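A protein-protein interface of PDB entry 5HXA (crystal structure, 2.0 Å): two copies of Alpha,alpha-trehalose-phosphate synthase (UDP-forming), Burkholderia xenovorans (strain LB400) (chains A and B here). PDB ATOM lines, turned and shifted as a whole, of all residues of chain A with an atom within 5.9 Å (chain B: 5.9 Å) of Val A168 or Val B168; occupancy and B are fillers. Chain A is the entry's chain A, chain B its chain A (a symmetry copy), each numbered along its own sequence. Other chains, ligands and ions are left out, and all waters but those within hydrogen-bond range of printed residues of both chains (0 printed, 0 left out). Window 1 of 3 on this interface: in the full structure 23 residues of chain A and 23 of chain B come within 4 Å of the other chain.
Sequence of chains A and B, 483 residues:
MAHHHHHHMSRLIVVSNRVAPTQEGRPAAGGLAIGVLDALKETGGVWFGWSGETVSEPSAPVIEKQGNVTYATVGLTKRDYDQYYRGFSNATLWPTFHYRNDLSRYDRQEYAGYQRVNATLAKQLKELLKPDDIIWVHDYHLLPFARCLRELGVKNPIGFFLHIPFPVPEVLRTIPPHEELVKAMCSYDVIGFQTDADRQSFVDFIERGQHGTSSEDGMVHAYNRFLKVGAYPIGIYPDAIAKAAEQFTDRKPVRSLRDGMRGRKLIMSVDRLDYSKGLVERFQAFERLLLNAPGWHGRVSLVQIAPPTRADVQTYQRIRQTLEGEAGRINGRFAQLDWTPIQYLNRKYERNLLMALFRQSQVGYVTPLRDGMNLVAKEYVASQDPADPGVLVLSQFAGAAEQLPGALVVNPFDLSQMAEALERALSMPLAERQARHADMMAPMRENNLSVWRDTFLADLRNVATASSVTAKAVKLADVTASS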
ATOM      1  N   TYR A  99     -34.132  30.603 -11.547  1.00  0.00           N
ATOM      2  CA  TYR A  99     -34.034  29.171 -11.259  1.00  0.00           C
ATOM      3  C   TYR A  99     -35.005  28.743 -10.162  1.00  0.00           C
ATOM      4  O   TYR A  99     -34.719  27.834  -9.372  1.00  0.00           O
ATOM      5  CB  TYR A  99     -32.589  28.779 -10.914  1.00  0.00           C
ATOM      6  CG  TYR A  99     -31.701  28.737 -12.147  1.00  0.00           C
ATOM      7  CD1 TYR A  99     -31.259  29.916 -12.757  1.00  0.00           C
ATOM      8  CD2 TYR A  99     -31.328  27.525 -12.718  1.00  0.00           C
ATOM      9  CE1 TYR A  99     -30.453  29.883 -13.894  1.00  0.00           C
ATOM     10  CE2 TYR A  99     -30.526  27.482 -13.859  1.00  0.00           C
ATOM     11  CZ  TYR A  99     -30.092  28.661 -14.442  1.00  0.00           C
ATOM     12  OH  TYR A  99     -29.303  28.618 -15.572  1.00  0.00           O
ATOM     13  N   PHE A 166     -30.052  34.550 -17.569  1.00  0.00           N
ATOM     14  CA  PHE A 166     -30.811  33.877 -18.620  1.00  0.00           C
ATOM     15  C   PHE A 166     -30.708  32.375 -18.392  1.00  0.00           C
ATOM     16  O   PHE A 166     -29.613  31.810 -18.527  1.00  0.00           O
ATOM     17  CB  PHE A 166     -30.318  34.244 -20.027  1.00  0.00           C
ATOM     18  CG  PHE A 166     -31.271  33.796 -21.113  1.00  0.00           C
ATOM     19  CD1 PHE A 166     -32.403  34.553 -21.412  1.00  0.00           C
ATOM     20  CD2 PHE A 166     -31.078  32.586 -21.785  1.00  0.00           C
ATOM     21  CE1 PHE A 166     -33.314  34.138 -22.393  1.00  0.00           C
ATOM     22  CE2 PHE A 166     -31.987  32.161 -22.763  1.00  0.00           C
ATOM     23  CZ  PHE A 166     -33.108  32.950 -23.068  1.00  0.00           C
ATOM     24  N   PRO A 167     -31.798  31.692 -18.038  1.00  0.00           N
ATOM     25  CA  PRO A 167     -31.675  30.316 -17.557  1.00  0.00           C
ATOM     26  C   PRO A 167     -31.363  29.346 -18.688  1.00  0.00           C
ATOM     27  O   PRO A 167     -31.760  29.544 -19.840  1.00  0.00           O
ATOM     28  CB  PRO A 167     -33.056  30.034 -16.940  1.00  0.00           C
ATOM     29  CG  PRO A 167     -34.006  30.870 -17.794  1.00  0.00           C
ATOM     30  CD  PRO A 167     -33.204  32.162 -18.042  1.00  0.00           C
ATOM     31  N   VAL A 168     -30.653  28.275 -18.339  1.00  0.00           N
ATOM     32  CA  VAL A 168     -30.225  27.270 -19.317  1.00  0.00           C
ATOM     33  C   VAL A 168     -31.460  26.615 -19.932  1.00  0.00           C
ATOM     34  O   VAL A 168     -32.560  26.719 -19.362  1.00  0.00           O
ATOM     35  CB  VAL A 168     -29.282  26.234 -18.674  1.00  0.00           C
ATOM     36  CG1 VAL A 168     -27.939  26.898 -18.279  1.00  0.00           C
ATOM     37  CG2 VAL A 168     -29.929  25.588 -17.485  1.00  0.00           C
ATOM     38  N   PRO A 169     -31.330  25.957 -21.092  1.00  0.00           N
ATOM     39  CA  PRO A 169     -32.520  25.434 -21.790  1.00  0.00           C
ATOM     40  C   PRO A 169     -33.426  24.532 -20.960  1.00  0.00           C
ATOM     41  O   PRO A 169     -34.650  24.663 -21.071  1.00  0.00           O
ATOM     42  CB  PRO A 169     -31.902  24.673 -22.979  1.00  0.00           C
ATOM     43  CG  PRO A 169     -30.673  25.487 -23.309  1.00  0.00           C
ATOM     44  CD  PRO A 169     -30.126  25.903 -21.949  1.00  0.00           C
ATOM     45  N   GLU A 170     -32.881  23.610 -20.154  1.00  0.00           N
ATOM     46  CA  GLU A 170     -33.746  22.728 -19.366  1.00  0.00           C
ATOM     47  C   GLU A 170     -34.696  23.511 -18.471  1.00  0.00           C
ATOM     48  O   GLU A 170     -35.779  23.016 -18.142  1.00  0.00           O
ATOM     49  CB  GLU A 170     -32.920  21.769 -18.504  1.00  0.00           C
ATOM     50  CG  GLU A 170     -32.294  20.602 -19.272  1.00  0.00           C
ATOM     51  CD  GLU A 170     -33.337  19.652 -19.854  1.00  0.00           C
ATOM     52  OE1 GLU A 170     -34.496  19.593 -19.359  1.00  0.00           O
ATOM     53  OE2 GLU A 170     -32.977  18.936 -20.798  1.00  0.00           O
ATOM     54  N   VAL A 171     -34.296  24.708 -18.048  1.00  0.00           N
ATOM     55  CA  VAL A 171     -35.112  25.544 -17.170  1.00  0.00           C
ATOM     56  C   VAL A 171     -35.970  26.505 -17.975  1.00  0.00           C
ATOM     57  O   VAL A 171     -37.158  26.666 -17.683  1.00  0.00           O
ATOM     58  CB  VAL A 171     -34.210  26.292 -16.166  1.00  0.00           C
ATOM     59  CG1 VAL A 171     -35.005  27.352 -15.371  1.00  0.00           C
ATOM     60  CG2 VAL A 171     -33.536  25.296 -15.221  1.00  0.00           C
ATOM     61  N   LEU A 172     -35.373  27.144 -18.989  1.00  0.00           N
ATOM     62  CA  LEU A 172     -36.120  28.038 -19.872  1.00  0.00           C
ATOM     63  C   LEU A 172     -37.341  27.357 -20.482  1.00  0.00           C
ATOM     64  O   LEU A 172     -38.401  27.980 -20.623  1.00  0.00           O
ATOM     65  CB  LEU A 172     -35.208  28.547 -20.998  1.00  0.00           C
ATOM     66  CG  LEU A 172     -35.870  29.516 -21.987  1.00  0.00           C
ATOM     67  CD1 LEU A 172     -36.041  30.863 -21.319  1.00  0.00           C
ATOM     68  CD2 LEU A 172     -35.046  29.644 -23.259  1.00  0.00           C
ATOM     69  N   ARG A 173     -37.207  26.084 -20.873  1.00  0.00           N
ATOM     70  CA  ARG A 173     -38.300  25.439 -21.592  1.00  0.00           C
ATOM     71  C   ARG A 173     -39.510  25.162 -20.708  1.00  0.00           C
ATOM     72  O   ARG A 173     -40.561  24.777 -21.237  1.00  0.00           O
ATOM     73  CB  ARG A 173     -37.816  24.143 -22.261  1.00  0.00           C
ATOM     74  CG  ARG A 173     -37.419  22.990 -21.328  1.00  0.00           C
ATOM     75  CD  ARG A 173     -36.659  21.902 -22.125  1.00  0.00           C
ATOM     76  NE  ARG A 173     -36.452  20.662 -21.377  1.00  0.00           N
ATOM     77  CZ  ARG A 173     -37.209  19.575 -21.506  1.00  0.00           C
ATOM     78  NH1 ARG A 173     -38.228  19.570 -22.358  1.00  0.00           N
ATOM     79  NH2 ARG A 173     -36.957  18.494 -20.781  1.00  0.00           N
ATOM     80  N   ALA A 197     -21.849  32.868 -18.857  1.00  0.00           N
ATOM     81  CA  ALA A 197     -22.767  31.740 -18.689  1.00  0.00           C
ATOM     82  C   ALA A 197     -24.160  32.083 -19.211  1.00  0.00           C
ATOM     83  O   ALA A 197     -24.835  31.231 -19.797  1.00  0.00           O
ATOM     84  CB  ALA A 197     -22.837  31.319 -17.215  1.00  0.00           C
ATOM     85  N   SER A 201     -25.909  30.180 -22.284  1.00  0.00           N
ATOM     86  CA  SER A 201     -27.250  29.635 -22.108  1.00  0.00           C
ATOM     87  C   SER A 201     -28.155  29.989 -23.285  1.00  0.00           C
ATOM     88  O   SER A 201     -28.902  29.142 -23.792  1.00  0.00           O
ATOM     89  CB  SER A 201     -27.834  30.176 -20.804  1.00  0.00           C
ATOM     90  OG  SER A 201     -29.214  29.928 -20.732  1.00  0.00           O
ATOM     91  N   TYR B  99     -34.380  18.788 -10.264  1.00  0.00           N
ATOM     92  CA  TYR B  99     -34.506  20.225 -10.517  1.00  0.00           C
ATOM     93  C   TYR B  99     -35.309  20.927  -9.426  1.00  0.00           C
ATOM     94  O   TYR B  99     -36.024  21.903  -9.685  1.00  0.00           O
ATOM     95  CB  TYR B  99     -35.103  20.485 -11.909  1.00  0.00           C
ATOM     96  CG  TYR B  99     -34.093  20.233 -13.017  1.00  0.00           C
ATOM     97  CD1 TYR B  99     -33.740  18.931 -13.388  1.00  0.00           C
ATOM     98  CD2 TYR B  99     -33.472  21.291 -13.672  1.00  0.00           C
ATOM     99  CE1 TYR B  99     -32.808  18.694 -14.397  1.00  0.00           C
ATOM    100  CE2 TYR B  99     -32.533  21.064 -14.679  1.00  0.00           C
ATOM    101  CZ  TYR B  99     -32.205  19.767 -15.037  1.00  0.00           C
ATOM    102  OH  TYR B  99     -31.275  19.544 -16.029  1.00  0.00           O
ATOM    103  N   PHE B 166     -29.901  13.514 -14.803  1.00  0.00           N
ATOM    104  CA  PHE B 166     -28.637  14.109 -14.375  1.00  0.00           C
ATOM    105  C   PHE B 166     -28.697  15.604 -14.656  1.00  0.00           C
ATOM    106  O   PHE B 166     -28.733  16.006 -15.828  1.00  0.00           O
ATOM    107  CB  PHE B 166     -27.424  13.477 -15.073  1.00  0.00           C
ATOM    108  CG  PHE B 166     -26.113  13.870 -14.430  1.00  0.00           C
ATOM    109  CD1 PHE B 166     -25.672  13.220 -13.277  1.00  0.00           C
ATOM    110  CD2 PHE B 166     -25.356  14.932 -14.930  1.00  0.00           C
ATOM    111  CE1 PHE B 166     -24.476  13.591 -12.649  1.00  0.00           C
ATOM    112  CE2 PHE B 166     -24.161  15.313 -14.304  1.00  0.00           C
ATOM    113  CZ  PHE B 166     -23.721  14.630 -13.159  1.00  0.00           C
ATOM    114  N   PRO B 167     -28.723  16.460 -13.632  1.00  0.00           N
ATOM    115  CA  PRO B 167     -29.049  17.867 -13.865  1.00  0.00           C
ATOM    116  C   PRO B 167     -27.902  18.611 -14.534  1.00  0.00           C
ATOM    117  O   PRO B 167     -26.724  18.293 -14.345  1.00  0.00           O
ATOM    118  CB  PRO B 167     -29.315  18.405 -12.447  1.00  0.00           C
ATOM    119  CG  PRO B 167     -28.385  17.572 -11.569  1.00  0.00           C
ATOM    120  CD  PRO B 167     -28.475  16.170 -12.201  1.00  0.00           C
ATOM    121  N   VAL B 168     -28.262  19.628 -15.314  1.00  0.00           N
ATOM    122  CA  VAL B 168     -27.284  20.416 -16.072  1.00  0.00           C
ATOM    123  C   VAL B 168     -26.343  21.116 -15.094  1.00  0.00           C
ATOM    124  O   VAL B 168     -26.671  21.233 -13.901  1.00  0.00           O
ATOM    125  CB  VAL B 168     -27.982  21.414 -17.015  1.00  0.00           C
ATOM    126  CG1 VAL B 168     -28.734  20.658 -18.140  1.00  0.00           C
ATOM    127  CG2 VAL B 168     -28.917  22.304 -16.253  1.00  0.00           C
ATOM    128  N   PRO B 169     -25.167  21.571 -15.546  1.00  0.00           N
ATOM    129  CA  PRO B 169     -24.171  22.124 -14.608  1.00  0.00           C
ATOM    130  C   PRO B 169     -24.671  23.245 -13.703  1.00  0.00           C
ATOM    131  O   PRO B 169     -24.317  23.248 -12.519  1.00  0.00           O
ATOM    132  CB  PRO B 169     -23.059  22.617 -15.554  1.00  0.00           C
ATOM    133  CG  PRO B 169     -23.102  21.619 -16.688  1.00  0.00           C
ATOM    134  CD  PRO B 169     -24.587  21.349 -16.889  1.00  0.00           C
ATOM    135  N   GLU B 170     -25.456  24.203 -14.211  1.00  0.00           N
ATOM    136  CA  GLU B 170     -25.927  25.293 -13.351  1.00  0.00           C
ATOM    137  C   GLU B 170     -26.686  24.775 -12.139  1.00  0.00           C
ATOM    138  O   GLU B 170     -26.712  25.442 -11.099  1.00  0.00           O
ATOM    139  CB  GLU B 170     -26.823  26.262 -14.128  1.00  0.00           C
ATOM    140  CG  GLU B 170     -26.071  27.217 -15.060  1.00  0.00           C
ATOM    141  CD  GLU B 170     -25.168  28.187 -14.306  1.00  0.00           C
ATOM    142  OE1 GLU B 170     -25.391  28.461 -13.094  1.00  0.00           O
ATOM    143  OE2 GLU B 170     -24.242  28.704 -14.947  1.00  0.00           O
ATOM    144  N   VAL B 171     -27.327  23.615 -12.263  1.00  0.00           N
ATOM    145  CA  VAL B 171     -28.104  23.026 -11.175  1.00  0.00           C
ATOM    146  C   VAL B 171     -27.257  22.067 -10.356  1.00  0.00           C
ATOM    147  O   VAL B 171     -27.304  22.098  -9.125  1.00  0.00           O
ATOM    148  CB  VAL B 171     -29.363  22.333 -11.741  1.00  0.00           C
ATOM    149  CG1 VAL B 171     -30.091  21.510 -10.655  1.00  0.00           C
ATOM    150  CG2 VAL B 171     -30.302  23.371 -12.358  1.00  0.00           C
ATOM    151  N   LEU B 172     -26.481  21.215 -11.037  1.00  0.00           N
ATOM    152  CA  LEU B 172     -25.573  20.296 -10.352  1.00  0.00           C
ATOM    153  C   LEU B 172     -24.638  21.021  -9.392  1.00  0.00           C
ATOM    154  O   LEU B 172     -24.349  20.518  -8.298  1.00  0.00           O
ATOM    155  CB  LEU B 172     -24.740  19.516 -11.380  1.00  0.00           C
ATOM    156  CG  LEU B 172     -23.757  18.498 -10.787  1.00  0.00           C
ATOM    157  CD1 LEU B 172     -24.532  17.298 -10.288  1.00  0.00           C
ATOM    158  CD2 LEU B 172     -22.717  18.081 -11.815  1.00  0.00           C
ATOM    159  N   ARG B 173     -24.132  22.195  -9.789  1.00  0.00           N
ATOM    160  CA  ARG B 173     -23.122  22.853  -8.967  1.00  0.00           C
ATOM    161  C   ARG B 173     -23.685  23.405  -7.664  1.00  0.00           C
ATOM    162  O   ARG B 173     -22.900  23.832  -6.806  1.00  0.00           O
ATOM    163  CB  ARG B 173     -22.421  23.965  -9.762  1.00  0.00           C
ATOM    164  CG  ARG B 173     -23.269  25.189 -10.137  1.00  0.00           C
ATOM    165  CD  ARG B 173     -22.527  26.043 -11.194  1.00  0.00           C
ATOM    166  NE  ARG B 173     -23.146  27.348 -11.434  1.00  0.00           N
ATOM    167  CZ  ARG B 173     -22.726  28.487 -10.888  1.00  0.00           C
ATOM    168  NH1 ARG B 173     -21.681  28.488 -10.068  1.00  0.00           N
ATOM    169  NH2 ARG B 173     -23.351  29.625 -11.154  1.00  0.00           N
ATOM    170  N   ALA B 197     -30.209  13.972 -23.258  1.00  0.00           N
ATOM    171  CA  ALA B 197     -30.037  15.216 -22.504  1.00  0.00           C
ATOM    172  C   ALA B 197     -29.274  14.970 -21.205  1.00  0.00           C
ATOM    173  O   ALA B 197     -28.458  15.801 -20.794  1.00  0.00           O
ATOM    174  CB  ALA B 197     -31.400  15.859 -22.211  1.00  0.00           C
ATOM    175  N   SER B 201     -25.689  16.589 -20.399  1.00  0.00           N
ATOM    176  CA  SER B 201     -25.505  17.313 -19.146  1.00  0.00           C
ATOM    177  C   SER B 201     -24.213  16.899 -18.446  1.00  0.00           C
ATOM    178  O   SER B 201     -23.459  17.746 -17.949  1.00  0.00           O
ATOM    179  CB  SER B 201     -26.710  17.050 -18.243  1.00  0.00           C
ATOM    180  OG  SER B 201     -26.453  17.472 -16.929  1.00  0.00           O
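Pro A167 touches none of the printed residues of chain B.
Val A168 touches two residues of chain B.
Printed residues of chain B within 4 Å of Glu A170: Tyr B99 (3.6 Å), Val B168 (3.7 Å) and Ala B197 (3.7 Å).
Of the printed residues of chain B, Ala A197 touches Glu B170.
Of the printed residues of chain A, Tyr B99 touches Glu A170.
Val B168 touches just these residues of chain A: Val A168 (3.7 Å) and Glu A170 (3.7 Å).
Of the printed residues of chain A, Glu B170 touches Tyr A99 (3.6 Å), Val A168 (3.7 Å) and Ala A197 (3.7 Å).
Ser B201 touches none of the printed residues of chain A.
Of the 11 printed residues of chain A, 4 touch a printed residue of chain B.
Among the printed residues, 7 pairs touch across the chains.
Among the printed residues, no Asp or Glu carboxylate lies within 4 Å of a Lys or Arg side-chain nitrogen of the other chain.
Among the printed residues, merely in contact across the chains: Tyr A99 with Glu B170 (3.6 Å), Val A168 with Val B168 (3.7 Å), Val A168 with Glu B170 (3.7 Å), Glu A170 with Tyr B99 (3.6 Å), Glu A170 with Val B168 (3.7 Å), Glu A170 with Ala B197 (3.7 Å) and Ala A197 with Glu B170 (3.7 Å).
N of Val B168 is in hydrogen-bond range of OH of Tyr B99 (3.1 Å).
OG of Ser B201 sits close to N of Val B168, 3.2 Å away.
OE1 of Glu B170 is in salt-bridge range of NE of Arg B173.
The side-chain hydroxyl (OH) of Tyr A99 sits at hydrogen-bond distance from the backbone NH (N) of Val A168.
The side-chain carboxylate of Glu A170 is in salt-bridge range of the guanidinium group of Arg A173 (3.0 Å).
OG of Ser A201 sits close to N of Val A168.
Tyr A99 touches Glu B170, and with the chains exchanged Glu A170 touches Tyr B99.
Val A168 touches its own counterpart, Val B168.
Val A168 touches Glu B170, and with the chains exchanged Glu A170 touches Val B168.
Glu A170 touches Ala B197, and with the chains exchanged Ala A197 touches Glu B170.
Positions printed for both chains: 99, 166, 167, 168, 169, 170, 171, 172, 173, 197 and 201.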
